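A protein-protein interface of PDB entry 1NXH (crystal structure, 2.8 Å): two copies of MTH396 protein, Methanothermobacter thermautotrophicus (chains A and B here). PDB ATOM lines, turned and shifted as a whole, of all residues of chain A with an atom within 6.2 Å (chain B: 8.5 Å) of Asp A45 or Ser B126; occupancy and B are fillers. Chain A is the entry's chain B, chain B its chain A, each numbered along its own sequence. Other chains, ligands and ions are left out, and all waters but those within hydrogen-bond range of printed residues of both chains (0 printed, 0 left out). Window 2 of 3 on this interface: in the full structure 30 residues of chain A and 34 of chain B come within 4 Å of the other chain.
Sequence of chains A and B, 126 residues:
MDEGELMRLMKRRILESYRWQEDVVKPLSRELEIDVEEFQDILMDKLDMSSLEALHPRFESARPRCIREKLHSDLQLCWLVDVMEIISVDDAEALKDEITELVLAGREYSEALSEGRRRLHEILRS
Ile A42 touches Leu B124 (CG2 to O, 3.3 Å).
CD2 of Leu A43 touches CD1 of Ile B86, at 3.4 Å.
Ser B126 touches Asp A45 (OXT to OD1, 3.9 Å).
Ile B86 touches Lys A46.
CE of Lys A46 touches O of Ser B126 (3.8 Å).
Leu A47 touches Ile B86 (CD1 to CG1, 3.6 Å).
Of the 10 printed residues of chain B, 4 touch a printed residue of chain A.
Of the 9 printed residues of chain A, 5 touch a printed residue of chain B.
Printed residues of chain A that touch a printed residue of chain B: Ile A42, Leu A43, Asp A45, Lys A46 and Leu A47.
Hydrophobic or aromatic side chains of chain A within 4 Å of the printed part of chain B: Ile A42, Leu A43 and Leu A47.
Among the printed residues, no Asp or Glu carboxylate lies within 4 Å of a Lys or Arg side-chain nitrogen of the other chain.
The backbone carbonyl oxygen of Glu B122 is in hydrogen-bond range of the side-chain hydroxyl of Ser B126 (3.0 Å).
The backbone carbonyl oxygen (O) of Ile B123 lies close to the side-chain hydroxyl (OG) of Ser B126 (3.2 Å).
NZ of Lys A11 is in hydrogen-bond range of O of Leu A47, at 2.9 Å.
O of Ile B123 is in hydrogen-bond range of NZ of Lys A46, at 3.1 Å.
O of Leu B124 is in hydrogen-bond range of NZ of Lys A46, at 2.6 Å.
Printed residues of chain B within 4 Å of Leu A43: Ile B86.
Of chain B, only Ser B126 (3.9 Å) comes within 4 Å of Asp A45.
Printed residues of chain B within 4 Å of Leu A47: Ile B86.
Of the printed residues of chain A, Ile B86 touches Leu A43, Lys A46 and Leu A47.
The nearest residue of chain A that does not touch Ser B126 is Ile A42 (6.1 Å).
No position is printed for both chains.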
ATOM      1  N   LYS A  11     -12.485 -26.303 -27.311  1.00  0.00           N
ATOM      2  CA  LYS A  11     -13.771 -26.968 -27.152  1.00  0.00           C
ATOM      3  C   LYS A  11     -14.786 -26.450 -28.148  1.00  0.00           C
ATOM      4  O   LYS A  11     -15.557 -27.221 -28.718  1.00  0.00           O
ATOM      5  CB  LYS A  11     -14.308 -26.795 -25.732  1.00  0.00           C
ATOM      6  CG  LYS A  11     -14.655 -25.372 -25.328  1.00  0.00           C
ATOM      7  CD  LYS A  11     -15.356 -25.365 -23.960  1.00  0.00           C
ATOM      8  CE  LYS A  11     -14.564 -26.137 -22.882  1.00  0.00           C
ATOM      9  NZ  LYS A  11     -15.263 -26.128 -21.553  1.00  0.00           N
ATOM     10  N   GLN A  40     -25.453 -24.798 -27.130  1.00  0.00           N
ATOM     11  CA  GLN A  40     -24.023 -24.871 -27.348  1.00  0.00           C
ATOM     12  C   GLN A  40     -23.288 -24.149 -26.232  1.00  0.00           C
ATOM     13  O   GLN A  40     -22.368 -24.692 -25.625  1.00  0.00           O
ATOM     14  CB  GLN A  40     -23.672 -24.218 -28.677  1.00  0.00           C
ATOM     15  CG  GLN A  40     -23.942 -25.078 -29.877  1.00  0.00           C
ATOM     16  CD  GLN A  40     -22.659 -25.539 -30.535  1.00  0.00           C
ATOM     17  OE1 GLN A  40     -21.912 -24.732 -31.087  1.00  0.00           O
ATOM     18  NE2 GLN A  40     -22.388 -26.840 -30.473  1.00  0.00           N
ATOM     19  N   ASP A  41     -23.702 -22.916 -25.966  1.00  0.00           N
ATOM     20  CA  ASP A  41     -23.074 -22.105 -24.930  1.00  0.00           C
ATOM     21  C   ASP A  41     -23.252 -22.734 -23.562  1.00  0.00           C
ATOM     22  O   ASP A  41     -22.360 -22.676 -22.717  1.00  0.00           O
ATOM     23  CB  ASP A  41     -23.686 -20.709 -24.928  1.00  0.00           C
ATOM     24  CG  ASP A  41     -23.772 -20.123 -26.311  1.00  0.00           C
ATOM     25  OD1 ASP A  41     -22.723 -20.043 -26.984  1.00  0.00           O
ATOM     26  OD2 ASP A  41     -24.888 -19.750 -26.727  1.00  0.00           O
ATOM     27  N   ILE A  42     -24.417 -23.333 -23.359  1.00  0.00           N
ATOM     28  CA  ILE A  42     -24.738 -23.973 -22.100  1.00  0.00           C
ATOM     29  C   ILE A  42     -23.755 -25.090 -21.887  1.00  0.00           C
ATOM     30  O   ILE A  42     -23.190 -25.242 -20.804  1.00  0.00           O
ATOM     31  CB  ILE A  42     -26.137 -24.543 -22.145  1.00  0.00           C
ATOM     32  CG1 ILE A  42     -27.035 -23.580 -22.913  1.00  0.00           C
ATOM     33  CG2 ILE A  42     -26.676 -24.717 -20.745  1.00  0.00           C
ATOM     34  CD1 ILE A  42     -26.937 -22.147 -22.427  1.00  0.00           C
ATOM     35  N   LEU A  43     -23.562 -25.881 -22.932  1.00  0.00           N
ATOM     36  CA  LEU A  43     -22.608 -26.972 -22.864  1.00  0.00           C
ATOM     37  C   LEU A  43     -21.239 -26.348 -22.578  1.00  0.00           C
ATOM     38  O   LEU A  43     -20.526 -26.767 -21.660  1.00  0.00           O
ATOM     39  CB  LEU A  43     -22.578 -27.739 -24.190  1.00  0.00           C
ATOM     40  CG  LEU A  43     -23.802 -28.594 -24.534  1.00  0.00           C
ATOM     41  CD1 LEU A  43     -23.764 -28.969 -26.004  1.00  0.00           C
ATOM     42  CD2 LEU A  43     -23.821 -29.840 -23.666  1.00  0.00           C
ATOM     43  N   MET A  44     -20.894 -25.332 -23.367  1.00  0.00           N
ATOM     44  CA  MET A  44     -19.629 -24.623 -23.226  1.00  0.00           C
ATOM     45  C   MET A  44     -19.489 -24.219 -21.770  1.00  0.00           C
ATOM     46  O   MET A  44     -18.447 -24.411 -21.140  1.00  0.00           O
ATOM     47  CB  MET A  44     -19.639 -23.370 -24.105  1.00  0.00           C
ATOM     48  CG  MET A  44     -18.268 -22.968 -24.623  1.00  0.00           C
ATOM     49  SD  MET A  44     -17.779 -23.851 -26.273  1.00  0.00           S
ATOM     50  CE  MET A  44     -17.896 -25.676 -25.722  1.00  0.00           C
ATOM     51  N   ASP A  45     -20.583 -23.670 -21.256  1.00  0.00           N
ATOM     52  CA  ASP A  45     -20.714 -23.190 -19.882  1.00  0.00           C
ATOM     53  C   ASP A  45     -20.587 -24.289 -18.812  1.00  0.00           C
ATOM     54  O   ASP A  45     -19.867 -24.125 -17.824  1.00  0.00           O
ATOM     55  CB  ASP A  45     -22.076 -22.477 -19.757  1.00  0.00           C
ATOM     56  CG  ASP A  45     -22.400 -22.025 -18.343  1.00  0.00           C
ATOM     57  OD1 ASP A  45     -23.532 -21.532 -18.141  1.00  0.00           O
ATOM     58  OD2 ASP A  45     -21.544 -22.152 -17.441  1.00  0.00           O
ATOM     59  N   LYS A  46     -21.263 -25.415 -19.018  1.00  0.00           N
ATOM     60  CA  LYS A  46     -21.250 -26.490 -18.031  1.00  0.00           C
ATOM     61  C   LYS A  46     -20.088 -27.484 -18.041  1.00  0.00           C
ATOM     62  O   LYS A  46     -19.367 -27.621 -17.048  1.00  0.00           O
ATOM     63  CB  LYS A  46     -22.577 -27.247 -18.114  1.00  0.00           C
ATOM     64  CG  LYS A  46     -23.807 -26.381 -17.799  1.00  0.00           C
ATOM     65  CD  LYS A  46     -23.816 -25.943 -16.325  1.00  0.00           C
ATOM     66  CE  LYS A  46     -25.002 -25.024 -15.973  1.00  0.00           C
ATOM     67  NZ  LYS A  46     -26.342 -25.707 -15.975  1.00  0.00           N
ATOM     68  N   LEU A  47     -19.912 -28.181 -19.155  1.00  0.00           N
ATOM     69  CA  LEU A  47     -18.860 -29.182 -19.264  1.00  0.00           C
ATOM     70  C   LEU A  47     -17.458 -28.636 -19.471  1.00  0.00           C
ATOM     71  O   LEU A  47     -17.256 -27.671 -20.203  1.00  0.00           O
ATOM     72  CB  LEU A  47     -19.215 -30.161 -20.378  1.00  0.00           C
ATOM     73  CG  LEU A  47     -20.371 -31.062 -19.944  1.00  0.00           C
ATOM     74  CD1 LEU A  47     -21.398 -31.197 -21.055  1.00  0.00           C
ATOM     75  CD2 LEU A  47     -19.811 -32.409 -19.515  1.00  0.00           C
ATOM     76  N   ILE B  86     -24.762 -32.822 -17.136  1.00  0.00           N
ATOM     77  CA  ILE B  86     -24.899 -31.377 -17.225  1.00  0.00           C
ATOM     78  C   ILE B  86     -25.739 -30.898 -16.036  1.00  0.00           C
ATOM     79  O   ILE B  86     -25.666 -29.732 -15.626  1.00  0.00           O
ATOM     80  CB  ILE B  86     -25.637 -30.997 -18.508  1.00  0.00           C
ATOM     81  CG1 ILE B  86     -24.790 -31.361 -19.719  1.00  0.00           C
ATOM     82  CG2 ILE B  86     -26.000 -29.530 -18.495  1.00  0.00           C
ATOM     83  CD1 ILE B  86     -25.529 -31.168 -21.026  1.00  0.00           C
ATOM     84  N   ASP B  91     -30.468 -31.724  -8.353  1.00  0.00           N
ATOM     85  CA  ASP B  91     -31.324 -30.831  -9.129  1.00  0.00           C
ATOM     86  C   ASP B  91     -32.435 -31.653  -9.785  1.00  0.00           C
ATOM     87  O   ASP B  91     -33.635 -31.379  -9.605  1.00  0.00           O
ATOM     88  CB  ASP B  91     -30.523 -30.127 -10.234  1.00  0.00           C
ATOM     89  CG  ASP B  91     -29.688 -28.969  -9.722  1.00  0.00           C
ATOM     90  OD1 ASP B  91     -28.845 -28.472 -10.502  1.00  0.00           O
ATOM     91  OD2 ASP B  91     -29.875 -28.553  -8.556  1.00  0.00           O
ATOM     92  N   ARG B 119     -38.469 -24.594 -15.828  1.00  0.00           N
ATOM     93  CA  ARG B 119     -37.546 -24.637 -14.708  1.00  0.00           C
ATOM     94  C   ARG B 119     -36.252 -25.348 -15.083  1.00  0.00           C
ATOM     95  O   ARG B 119     -35.212 -25.094 -14.488  1.00  0.00           O
ATOM     96  CB  ARG B 119     -38.192 -25.291 -13.490  1.00  0.00           C
ATOM     97  CG  ARG B 119     -37.694 -24.661 -12.175  1.00  0.00           C
ATOM     98  CD  ARG B 119     -38.502 -25.128 -10.974  1.00  0.00           C
ATOM     99  NE  ARG B 119     -39.925 -25.223 -11.306  1.00  0.00           N
ATOM    100  CZ  ARG B 119     -40.897 -25.488 -10.432  1.00  0.00           C
ATOM    101  NH1 ARG B 119     -40.610 -25.685  -9.151  1.00  0.00           N
ATOM    102  NH2 ARG B 119     -42.161 -25.564 -10.843  1.00  0.00           N
ATOM    103  N   LEU B 120     -36.316 -26.226 -16.077  1.00  0.00           N
ATOM    104  CA  LEU B 120     -35.129 -26.939 -16.535  1.00  0.00           C
ATOM    105  C   LEU B 120     -34.180 -25.946 -17.169  1.00  0.00           C
ATOM    106  O   LEU B 120     -33.039 -25.794 -16.731  1.00  0.00           O
ATOM    107  CB  LEU B 120     -35.486 -27.995 -17.581  1.00  0.00           C
ATOM    108  CG  LEU B 120     -34.235 -28.635 -18.209  1.00  0.00           C
ATOM    109  CD1 LEU B 120     -33.469 -29.352 -17.127  1.00  0.00           C
ATOM    110  CD2 LEU B 120     -34.601 -29.610 -19.321  1.00  0.00           C
ATOM    111  N   HIS B 121     -34.662 -25.295 -18.227  1.00  0.00           N
ATOM    112  CA  HIS B 121     -33.885 -24.285 -18.948  1.00  0.00           C
ATOM    113  C   HIS B 121     -33.219 -23.390 -17.926  1.00  0.00           C
ATOM    114  O   HIS B 121     -32.038 -23.053 -18.033  1.00  0.00           O
ATOM    115  CB  HIS B 121     -34.799 -23.439 -19.839  1.00  0.00           C
ATOM    116  CG  HIS B 121     -35.238 -24.138 -21.084  1.00  0.00           C
ATOM    117  ND1 HIS B 121     -34.367 -24.458 -22.104  1.00  0.00           N
ATOM    118  CD2 HIS B 121     -36.449 -24.611 -21.464  1.00  0.00           C
ATOM    119  CE1 HIS B 121     -35.021 -25.100 -23.057  1.00  0.00           C
ATOM    120  NE2 HIS B 121     -36.286 -25.206 -22.693  1.00  0.00           N
ATOM    121  N   GLU B 122     -34.001 -23.019 -16.922  1.00  0.00           N
ATOM    122  CA  GLU B 122     -33.519 -22.177 -15.850  1.00  0.00           C
ATOM    123  C   GLU B 122     -32.231 -22.787 -15.322  1.00  0.00           C
ATOM    124  O   GLU B 122     -31.162 -22.187 -15.408  1.00  0.00           O
ATOM    125  CB  GLU B 122     -34.571 -22.130 -14.752  1.00  0.00           C
ATOM    126  CG  GLU B 122     -34.403 -21.007 -13.777  1.00  0.00           C
ATOM    127  CD  GLU B 122     -35.741 -20.487 -13.321  1.00  0.00           C
ATOM    128  OE1 GLU B 122     -36.587 -21.331 -12.960  1.00  0.00           O
ATOM    129  OE2 GLU B 122     -35.950 -19.251 -13.329  1.00  0.00           O
ATOM    130  N   ILE B 123     -32.344 -24.000 -14.798  1.00  0.00           N
ATOM    131  CA  ILE B 123     -31.210 -24.720 -14.245  1.00  0.00           C
ATOM    132  C   ILE B 123     -30.033 -24.739 -15.202  1.00  0.00           C
ATOM    133  O   ILE B 123     -28.913 -24.386 -14.832  1.00  0.00           O
ATOM    134  CB  ILE B 123     -31.606 -26.171 -13.910  1.00  0.00           C
ATOM    135  CG1 ILE B 123     -32.675 -26.175 -12.816  1.00  0.00           C
ATOM    136  CG2 ILE B 123     -30.391 -26.954 -13.438  1.00  0.00           C
ATOM    137  CD1 ILE B 123     -33.303 -27.526 -12.589  1.00  0.00           C
ATOM    138  N   LEU B 124     -30.291 -25.156 -16.434  1.00  0.00           N
ATOM    139  CA  LEU B 124     -29.238 -25.223 -17.432  1.00  0.00           C
ATOM    140  C   LEU B 124     -28.497 -23.903 -17.522  1.00  0.00           C
ATOM    141  O   LEU B 124     -27.270 -23.872 -17.589  1.00  0.00           O
ATOM    142  CB  LEU B 124     -29.822 -25.577 -18.796  1.00  0.00           C
ATOM    143  CG  LEU B 124     -30.417 -26.982 -18.914  1.00  0.00           C
ATOM    144  CD1 LEU B 124     -30.989 -27.184 -20.314  1.00  0.00           C
ATOM    145  CD2 LEU B 124     -29.337 -28.025 -18.603  1.00  0.00           C
ATOM    146  N   ARG B 125     -29.249 -22.810 -17.523  1.00  0.00           N
ATOM    147  CA  ARG B 125     -28.657 -21.485 -17.604  1.00  0.00           C
ATOM    148  C   ARG B 125     -28.310 -20.955 -16.205  1.00  0.00           C
ATOM    149  O   ARG B 125     -28.789 -19.899 -15.798  1.00  0.00           O
ATOM    150  CB  ARG B 125     -29.635 -20.533 -18.283  1.00  0.00           C
ATOM    151  CG  ARG B 125     -30.183 -21.014 -19.619  1.00  0.00           C
ATOM    152  CD  ARG B 125     -31.423 -20.198 -19.986  1.00  0.00           C
ATOM    153  NE  ARG B 125     -31.967 -20.487 -21.312  1.00  0.00           N
ATOM    154  CZ  ARG B 125     -33.170 -20.087 -21.715  1.00  0.00           C
ATOM    155  NH1 ARG B 125     -33.938 -19.393 -20.882  1.00  0.00           N
ATOM    156  NH2 ARG B 125     -33.603 -20.360 -22.943  1.00  0.00           N
ATOM    157  N   SER B 126     -27.484 -21.694 -15.471  1.00  0.00           N
ATOM    158  CA  SER B 126     -27.084 -21.289 -14.128  1.00  0.00           C
ATOM    159  C   SER B 126     -25.608 -21.570 -13.893  1.00  0.00           C
ATOM    160  O   SER B 126     -25.312 -22.502 -13.111  1.00  0.00           O
ATOM    161  CB  SER B 126     -27.905 -22.032 -13.080  1.00  0.00           C
ATOM    162  OG  SER B 126     -29.268 -21.689 -13.173  1.00  0.00           O
ATOM    163  OXT SER B 126     -24.765 -20.863 -14.491  1.00  0.00           O
